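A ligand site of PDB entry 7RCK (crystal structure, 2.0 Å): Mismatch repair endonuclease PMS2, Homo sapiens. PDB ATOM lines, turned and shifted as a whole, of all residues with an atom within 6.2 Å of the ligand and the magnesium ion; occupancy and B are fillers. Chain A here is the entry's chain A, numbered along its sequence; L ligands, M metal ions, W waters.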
ATOM      1  N   GLU A  41     -13.157  25.266  -9.181  1.00  0.00           N
ATOM      2  CA  GLU A  41     -11.818  25.351  -9.773  1.00  0.00           C
ATOM      3  C   GLU A  41     -11.035  24.075  -9.542  1.00  0.00           C
ATOM      4  O   GLU A  41     -10.362  23.579 -10.458  1.00  0.00           O
ATOM      5  CB  GLU A  41     -11.063  26.545  -9.203  1.00  0.00           C
ATOM      6  CG  GLU A  41     -11.647  27.919  -9.507  1.00  0.00           C
ATOM      7  CD  GLU A  41     -11.580  28.291 -10.977  1.00  0.00           C
ATOM      8  OE1 GLU A  41     -10.778  27.688 -11.721  1.00  0.00           O
ATOM      9  OE2 GLU A  41     -12.331  29.207 -11.384  1.00  0.00           O
ATOM     10  N   LEU A  42     -11.108  23.522  -8.328  1.00  0.00           N
ATOM     11  CA  LEU A  42     -10.353  22.303  -8.016  1.00  0.00           C
ATOM     12  C   LEU A  42     -10.913  21.101  -8.773  1.00  0.00           C
ATOM     13  O   LEU A  42     -10.146  20.249  -9.238  1.00  0.00           O
ATOM     14  CB  LEU A  42     -10.365  22.055  -6.515  1.00  0.00           C
ATOM     15  CG  LEU A  42      -9.718  23.140  -5.649  1.00  0.00           C
ATOM     16  CD1 LEU A  42      -9.914  22.838  -4.175  1.00  0.00           C
ATOM     17  CD2 LEU A  42      -8.242  23.293  -5.978  1.00  0.00           C
ATOM     18  N   GLU A  44     -12.544  21.173 -11.679  1.00  0.00           N
ATOM     19  CA  GLU A  44     -12.157  21.346 -13.078  1.00  0.00           C
ATOM     20  C   GLU A  44     -10.693  20.977 -13.291  1.00  0.00           C
ATOM     21  O   GLU A  44     -10.340  20.400 -14.328  1.00  0.00           O
ATOM     22  CB  GLU A  44     -12.425  22.776 -13.529  1.00  0.00           C
ATOM     23  CG  GLU A  44     -13.889  23.109 -13.746  1.00  0.00           C
ATOM     24  CD  GLU A  44     -14.376  22.715 -15.129  1.00  0.00           C
ATOM     25  OE1 GLU A  44     -13.537  22.599 -16.048  1.00  0.00           O
ATOM     26  OE2 GLU A  44     -15.602  22.535 -15.301  1.00  0.00           O
ATOM     27  N   ASN A  45      -9.820  21.311 -12.340  1.00  0.00           N
ATOM     28  CA  ASN A  45      -8.414  20.947 -12.469  1.00  0.00           C
ATOM     29  C   ASN A  45      -8.239  19.430 -12.472  1.00  0.00           C
ATOM     30  O   ASN A  45      -7.446  18.898 -13.253  1.00  0.00           O
ATOM     31  CB  ASN A  45      -7.599  21.579 -11.335  1.00  0.00           C
ATOM     32  CG  ASN A  45      -7.357  23.053 -11.546  1.00  0.00           C
ATOM     33  OD1 ASN A  45      -7.494  23.565 -12.661  1.00  0.00           O
ATOM     34  ND2 ASN A  45      -6.987  23.760 -10.483  1.00  0.00           N
ATOM     35  N   SER A  46      -8.958  18.724 -11.595  1.00  0.00           N
ATOM     36  CA  SER A  46      -8.889  17.265 -11.588  1.00  0.00           C
ATOM     37  C   SER A  46      -9.447  16.680 -12.878  1.00  0.00           C
ATOM     38  O   SER A  46      -8.894  15.709 -13.417  1.00  0.00           O
ATOM     39  CB  SER A  46      -9.632  16.715 -10.374  1.00  0.00           C
ATOM     40  OG  SER A  46      -9.019  17.134  -9.166  1.00  0.00           O
ATOM     41  N   ASP A  48      -9.487  18.247 -15.793  1.00  0.00           N
ATOM     42  CA  ASP A  48      -8.515  18.581 -16.830  1.00  0.00           C
ATOM     43  C   ASP A  48      -7.328  17.622 -16.806  1.00  0.00           C
ATOM     44  O   ASP A  48      -6.721  17.363 -17.855  1.00  0.00           O
ATOM     45  CB  ASP A  48      -8.021  20.017 -16.664  1.00  0.00           C
ATOM     46  CG  ASP A  48      -9.066  21.048 -17.053  1.00  0.00           C
ATOM     47  OD1 ASP A  48     -10.020  20.684 -17.791  1.00  0.00           O
ATOM     48  OD2 ASP A  48      -8.942  22.212 -16.634  1.00  0.00           O
ATOM     49  N   ALA A  49      -6.986  17.090 -15.638  1.00  0.00           N
ATOM     50  CA  ALA A  49      -5.871  16.164 -15.510  1.00  0.00           C
ATOM     51  C   ALA A  49      -6.222  14.744 -15.924  1.00  0.00           C
ATOM     52  O   ALA A  49      -5.382  13.849 -15.792  1.00  0.00           O
ATOM     53  CB  ALA A  49      -5.367  16.157 -14.060  1.00  0.00           C
ATOM     54  N   ASP A  70      -7.392  13.315  -6.521  1.00  0.00           N
ATOM     55  CA  ASP A  70      -7.690  12.717  -7.815  1.00  0.00           C
ATOM     56  C   ASP A  70      -6.565  11.767  -8.213  1.00  0.00           C
ATOM     57  O   ASP A  70      -5.457  11.818  -7.668  1.00  0.00           O
ATOM     58  CB  ASP A  70      -7.916  13.783  -8.909  1.00  0.00           C
ATOM     59  CG  ASP A  70      -6.653  14.570  -9.241  1.00  0.00           C
ATOM     60  OD1 ASP A  70      -5.699  13.989  -9.798  1.00  0.00           O
ATOM     61  OD2 ASP A  70      -6.626  15.790  -8.978  1.00  0.00           O
ATOM     62  N   GLY A  72      -5.477  11.755 -11.422  1.00  0.00           N
ATOM     63  CA  GLY A  72      -5.134  12.322 -12.708  1.00  0.00           C
ATOM     64  C   GLY A  72      -3.657  12.209 -13.037  1.00  0.00           C
ATOM     65  O   GLY A  72      -2.933  11.423 -12.428  1.00  0.00           O
ATOM     66  N   CYS A  73      -3.195  13.019 -14.002  1.00  0.00           N
ATOM     67  CA  CYS A  73      -1.829  12.889 -14.508  1.00  0.00           C
ATOM     68  C   CYS A  73      -0.771  13.359 -13.527  1.00  0.00           C
ATOM     69  O   CYS A  73       0.393  12.974 -13.657  1.00  0.00           O
ATOM     70  CB  CYS A  73      -1.683  13.666 -15.819  1.00  0.00           C
ATOM     71  SG  CYS A  73      -1.984  15.451 -15.677  1.00  0.00           S
ATOM     72  N   GLY A  74      -1.135  14.181 -12.546  1.00  0.00           N
ATOM     73  CA  GLY A  74      -0.160  14.724 -11.628  1.00  0.00           C
ATOM     74  C   GLY A  74       0.640  15.857 -12.257  1.00  0.00           C
ATOM     75  O   GLY A  74       0.433  16.265 -13.401  1.00  0.00           O
ATOM     76  N   VAL A  75       1.605  16.361 -11.476  1.00  0.00           N
ATOM     77  CA  VAL A  75       2.429  17.500 -11.883  1.00  0.00           C
ATOM     78  C   VAL A  75       3.884  17.059 -11.870  1.00  0.00           C
ATOM     79  O   VAL A  75       4.352  16.457 -10.906  1.00  0.00           O
ATOM     80  CB  VAL A  75       2.217  18.707 -10.953  1.00  0.00           C
ATOM     81  CG1 VAL A  75       2.974  19.918 -11.478  1.00  0.00           C
ATOM     82  CG2 VAL A  75       0.732  19.016 -10.801  1.00  0.00           C
ATOM     83  N   GLY A  82       5.738  26.628 -11.177  1.00  0.00           N
ATOM     84  CA  GLY A  82       4.731  27.180 -12.064  1.00  0.00           C
ATOM     85  C   GLY A  82       3.309  26.970 -11.604  1.00  0.00           C
ATOM     86  O   GLY A  82       2.390  27.535 -12.223  1.00  0.00           O
ATOM     87  N   LEU A  83       3.095  26.183 -10.547  1.00  0.00           N
ATOM     88  CA  LEU A  83       1.745  25.994 -10.016  1.00  0.00           C
ATOM     89  C   LEU A  83       1.153  27.319  -9.556  1.00  0.00           C
ATOM     90  O   LEU A  83      -0.042  27.569  -9.741  1.00  0.00           O
ATOM     91  CB  LEU A  83       1.764  24.990  -8.874  1.00  0.00           C
ATOM     92  CG  LEU A  83       2.017  23.520  -9.233  1.00  0.00           C
ATOM     93  CD1 LEU A  83       2.298  22.702  -7.980  1.00  0.00           C
ATOM     94  CD2 LEU A  83       0.831  22.955  -9.994  1.00  0.00           C
ATOM     95  N   THR A  84       1.972  28.170  -8.946  1.00  0.00           N
ATOM     96  CA  THR A  84       1.513  29.467  -8.454  1.00  0.00           C
ATOM     97  C   THR A  84       2.233  30.604  -9.168  1.00  0.00           C
ATOM     98  O   THR A  84       1.788  31.749  -9.136  1.00  0.00           O
ATOM     99  CB  THR A  84       1.719  29.605  -6.946  1.00  0.00           C
ATOM    100  OG1 THR A  84       3.115  29.541  -6.643  1.00  0.00           O
ATOM    101  CG2 THR A  84       0.997  28.481  -6.205  1.00  0.00           C
ATOM    102  N   GLU A 109      -4.485  33.328 -11.280  1.00  0.00           N
ATOM    103  CA  GLU A 109      -5.111  32.035 -11.526  1.00  0.00           C
ATOM    104  C   GLU A 109      -5.721  31.461 -10.249  1.00  0.00           C
ATOM    105  O   GLU A 109      -5.706  32.097  -9.201  1.00  0.00           O
ATOM    106  CB  GLU A 109      -4.094  31.050 -12.112  1.00  0.00           C
ATOM    107  CG  GLU A 109      -3.669  31.361 -13.534  1.00  0.00           C
ATOM    108  CD  GLU A 109      -4.750  31.055 -14.566  1.00  0.00           C
ATOM    109  OE1 GLU A 109      -5.746  31.802 -14.631  1.00  0.00           O
ATOM    110  OE2 GLU A 109      -4.595  30.059 -15.302  1.00  0.00           O
ATOM    111  N   ALA A 110      -6.253  30.245 -10.349  1.00  0.00           N
ATOM    112  CA  ALA A 110      -7.003  29.652  -9.238  1.00  0.00           C
ATOM    113  C   ALA A 110      -6.086  29.297  -8.074  1.00  0.00           C
ATOM    114  O   ALA A 110      -6.346  29.689  -6.928  1.00  0.00           O
ATOM    115  CB  ALA A 110      -7.773  28.417  -9.721  1.00  0.00           C
ATOM    116  N   LEU A 111      -5.017  28.540  -8.336  1.00  0.00           N
ATOM    117  CA  LEU A 111      -4.153  28.082  -7.257  1.00  0.00           C
ATOM    118  C   LEU A 111      -3.431  29.231  -6.577  1.00  0.00           C
ATOM    119  O   LEU A 111      -3.252  29.226  -5.356  1.00  0.00           O
ATOM    120  CB  LEU A 111      -3.160  27.046  -7.774  1.00  0.00           C
ATOM    121  CG  LEU A 111      -3.725  25.657  -8.058  1.00  0.00           C
ATOM    122  CD1 LEU A 111      -2.621  24.674  -8.418  1.00  0.00           C
ATOM    123  CD2 LEU A 111      -4.510  25.151  -6.847  1.00  0.00           C
ATOM    124  N   SER A 112      -3.015  30.242  -7.354  1.00  0.00           N
ATOM    125  CA  SER A 112      -2.351  31.396  -6.746  1.00  0.00           C
ATOM    126  C   SER A 112      -3.326  32.197  -5.886  1.00  0.00           C
ATOM    127  O   SER A 112      -2.956  32.688  -4.815  1.00  0.00           O
ATOM    128  CB  SER A 112      -1.739  32.278  -7.830  1.00  0.00           C
ATOM    129  OG  SER A 112      -2.737  32.852  -8.660  1.00  0.00           O
ATOM    130  N   THR A 124       1.625  15.422  -5.059  1.00  0.00           N
ATOM    131  CA  THR A 124       1.403  15.041  -6.446  1.00  0.00           C
ATOM    132  C   THR A 124       2.474  14.050  -6.871  1.00  0.00           C
ATOM    133  O   THR A 124       3.568  13.992  -6.306  1.00  0.00           O
ATOM    134  CB  THR A 124       1.398  16.268  -7.364  1.00  0.00           C
ATOM    135  OG1 THR A 124       0.973  15.894  -8.675  1.00  0.00           O
ATOM    136  CG2 THR A 124       2.790  16.889  -7.438  1.00  0.00           C
ATOM    137  N   GLY A 154      -1.356  11.081  -9.435  1.00  0.00           N
ATOM    138  CA  GLY A 154      -2.476  11.959  -9.203  1.00  0.00           C
ATOM    139  C   GLY A 154      -2.040  13.141  -8.375  1.00  0.00           C
ATOM    140  O   GLY A 154      -0.858  13.385  -8.169  1.00  0.00           O
ATOM    141  N   THR A 155      -3.036  13.883  -7.866  1.00  0.00           N
ATOM    142  CA  THR A 155      -2.772  15.112  -7.126  1.00  0.00           C
ATOM    143  C   THR A 155      -3.811  15.259  -6.019  1.00  0.00           C
ATOM    144  O   THR A 155      -4.988  14.947  -6.224  1.00  0.00           O
ATOM    145  CB  THR A 155      -2.818  16.334  -8.054  1.00  0.00           C
ATOM    146  OG1 THR A 155      -1.883  16.163  -9.131  1.00  0.00           O
ATOM    147  CG2 THR A 155      -2.470  17.611  -7.288  1.00  0.00           C
ATOM    148  N   THR A 156      -3.367  15.721  -4.863  1.00  0.00           N
ATOM    149  CA  THR A 156      -4.233  16.051  -3.739  1.00  0.00           C
ATOM    150  C   THR A 156      -3.981  17.494  -3.341  1.00  0.00           C
ATOM    151  O   THR A 156      -2.848  17.854  -2.995  1.00  0.00           O
ATOM    152  CB  THR A 156      -4.010  15.114  -2.552  1.00  0.00           C
ATOM    153  OG1 THR A 156      -4.336  13.777  -2.929  1.00  0.00           O
ATOM    154  CG2 THR A 156      -4.862  15.534  -1.372  1.00  0.00           C
ATOM    155  N   VAL A 157      -5.018  18.328  -3.396  1.00  0.00           N
ATOM    156  CA  VAL A 157      -4.927  19.737  -3.045  1.00  0.00           C
ATOM    157  C   VAL A 157      -5.727  19.968  -1.768  1.00  0.00           C
ATOM    158  O   VAL A 157      -6.931  19.672  -1.724  1.00  0.00           O
ATOM    159  CB  VAL A 157      -5.445  20.632  -4.180  1.00  0.00           C
ATOM    160  CG1 VAL A 157      -5.334  22.101  -3.791  1.00  0.00           C
ATOM    161  CG2 VAL A 157      -4.675  20.352  -5.469  1.00  0.00           C
HETATM  162  P1  LIG L   1      -7.903  27.982 -15.443  1.00  0.00           P
HETATM  163  O1  LIG L   1      -8.116  27.423 -14.054  1.00  0.00           O
HETATM  164  O2  LIG L   1      -8.758  27.219 -16.425  1.00  0.00           O
HETATM  165  O3  LIG L   1      -8.282  29.441 -15.466  1.00  0.00           O
HETATM  166  P2  LIG L   1      -5.250  26.869 -15.034  1.00  0.00           P
HETATM  167  O4  LIG L   1      -3.998  26.648 -15.858  1.00  0.00           O
HETATM  168  O5  LIG L   1      -5.889  25.522 -14.749  1.00  0.00           O
HETATM  169  O6  LIG L   1      -6.307  27.819 -15.865  1.00  0.00           O
HETATM  170  P3  LIG L   1      -4.883  26.860 -12.145  1.00  0.00           P
HETATM  171  O7  LIG L   1      -4.623  27.866 -11.046  1.00  0.00           O
HETATM  172  O8  LIG L   1      -6.247  26.204 -11.929  1.00  0.00           O
HETATM  173  O9  LIG L   1      -4.866  27.620 -13.600  1.00  0.00           O
HETATM  174  O10 LIG L   1      -3.665  25.687 -12.124  1.00  0.00           O
HETATM  175  C1  LIG L   1      -2.416  26.040 -12.664  1.00  0.00           C
HETATM  176  C2  LIG L   1      -1.725  24.766 -13.301  1.00  0.00           C
HETATM  177  O11 LIG L   1      -1.355  23.754 -12.182  1.00  0.00           O
HETATM  178  C3  LIG L   1      -2.544  24.141 -14.036  1.00  0.00           C
HETATM  179  O12 LIG L   1      -2.436  24.624 -15.426  1.00  0.00           O
HETATM  180  C4  LIG L   1      -2.068  22.548 -13.965  1.00  0.00           C
HETATM  181  O13 LIG L   1      -1.004  22.293 -14.937  1.00  0.00           O
HETATM  182  C5  LIG L   1      -1.640  22.349 -12.780  1.00  0.00           C
HETATM  183  N1  LIG L   1      -2.672  21.643 -11.962  1.00  0.00           N
HETATM  184  C6  LIG L   1      -3.515  22.269 -11.131  1.00  0.00           C
HETATM  185  N2  LIG L   1      -4.293  21.334 -10.555  1.00  0.00           N
HETATM  186  C7  LIG L   1      -3.930  20.143 -11.037  1.00  0.00           C
HETATM  187  C8  LIG L   1      -4.394  18.870 -10.792  1.00  0.00           C
HETATM  188  N3  LIG L   1      -5.496  18.399  -9.883  1.00  0.00           N
HETATM  189  N4  LIG L   1      -3.852  17.836 -11.422  1.00  0.00           N
HETATM  190  C9  LIG L   1      -2.827  18.035 -12.300  1.00  0.00           C
HETATM  191  N5  LIG L   1      -2.368  19.285 -12.545  1.00  0.00           N
HETATM  192  C10 LIG L   1      -2.925  20.337 -11.913  1.00  0.00           C
HETATM  193 MG    MG M   1      -7.679  25.499 -13.460  1.00  0.00          MG
HETATM  194  O   HOH W   1       1.758  21.275 -14.558  1.00  0.00           O
HETATM  195  O   HOH W   2      -5.185  20.227 -14.277  1.00  0.00           O
HETATM  196  O   HOH W   3      -9.487  29.592 -13.026  1.00  0.00           O
HETATM  197  O   HOH W   4      -9.354  25.696 -12.119  1.00  0.00           O
HETATM  198  O   HOH W   5      -1.330  21.966 -17.331  1.00  0.00           O
HETATM  199  O   HOH W   6      -8.970  24.496 -14.857  1.00  0.00           O
HETATM  200  O   HOH W   7      -5.794  22.769 -15.536  1.00  0.00           O
HETATM  201  O   HOH W   8      -6.532  17.422  -6.779  1.00  0.00           O
HETATM  202  O   HOH W   9      -3.472  15.039 -11.077  1.00  0.00           O
HETATM  203  O   HOH W  10      -7.530  19.830  -8.159  1.00  0.00           O
HETATM  204  O   HOH W  11      -0.380  19.044 -14.699  1.00  0.00           O
HETATM  205  O   HOH W  12      -6.166  22.104  -8.335  1.00  0.00           O
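The backbone NH (N) of Leu 111 is in hydrogen-bond range of an oxygen (O7) of the ligand, 2.8 Å away. The side-chain hydroxyl of Thr 155 sits at hydrogen-bond distance from a nitrogen (N4) of the ligand (3.5 Å). The backbone NH of Ala 110 sits at hydrogen-bond distance from an oxygen (O7) of the ligand (3.0 Å). OD2 of Asp 70 lies within hydrogen-bond range of N3 of the ligand (3.0 Å).
N of Val 75 is in hydrogen-bond range of OG1 of Thr 124 (2.9 Å). The backbone carbonyl oxygen (O) of Glu 109 sits at hydrogen-bond distance from the side-chain hydroxyl (OG) of Ser 112 (3.1 Å). N of Asp 70 lies within hydrogen-bond range of O of Thr 155 (2.9 Å). The backbone carbonyl oxygen (O) of Leu 42 is in hydrogen-bond range of the side-chain hydroxyl (OG) of Ser 46, at 3.3 Å. The side-chain hydroxyl (OG1) of Thr 124 lies within hydrogen-bond range of the side-chain hydroxyl (OG1) of Thr 155 (2.9 Å). The backbone carbonyl oxygen of Ala 49 is in hydrogen-bond range of the backbone NH of Cys 73, 2.9 Å away. The side-chain carboxylate of Asp 70 lies within hydrogen-bond range of the backbone NH of Gly 72, 2.8 Å away. OG of Ser 46 lies within hydrogen-bond range of OD2 of Asp 70, at 2.8 Å.
An oxygen (O6) of the ligand lies close to the side-chain carboxylate (OE2) of Glu 109 (2.9 Å). Glu 41 touches the ligand (OE1 to O1, 3.5 Å). OG of Ser 46 touches N3 of the ligand, 3.8 Å away. Ala 49 touches the ligand (CB to N4, 3.5 Å). Gly 74 touches the ligand. CG2 of Val 75 touches N5 of the ligand (3.6 Å). CD2 of Leu 83 touches O11 of the ligand (3.2 Å). Hydrophobic or aromatic side chains that line the ligand: Ala 49, Val 75, Leu 83, Ala 110 and Leu 111. The nearest printed residue that does not touch the ligand is Cys 73 (4.3 Å).
The nearest printed residue that does not touch the magnesium ion is Glu 41 (4.2 Å).
The magnesium ion is bound by O1 of the ligand, 2.1 Å away. OD1 of Asn 45 is bound to the magnesium ion (2.1 Å). The magnesium ion is bound by water W6 (2.2 Å). The magnesium ion is bound by water W4, at 2.2 Å. O5 of the ligand is bound to the magnesium ion, 2.2 Å away. O8 of the ligand binds the magnesium ion. The magnesium ion has six donor atoms within binding distance.
Water W4 bridges OE1 of Glu 41 (2.5 Å) and ND2 of Asn 45 (3.5 Å). Water W3 lies within hydrogen-bond range of OE1 of Glu 41 (2.6 Å) and O3 of the ligand (2.7 Å). Water W9 lies within hydrogen-bond range of OG1 of Thr 155 (2.8 Å), OD1 of Asp 70 (2.8 Å), N4 of the ligand (2.8 Å) and N of Gly 74 (2.9 Å). Water W12 bridges the side-chain amide nitrogen (ND2) of Asn 45 (2.8 Å) and a nitrogen (N2) of the ligand (3.0 Å). Water W10 lies within hydrogen-bond range of O of Leu 42 (2.9 Å), N3 of the ligand (3.0 Å) and OG of Ser 46 (3.2 Å). Water W2 bridges O of Asn 45 and N5 of the ligand.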
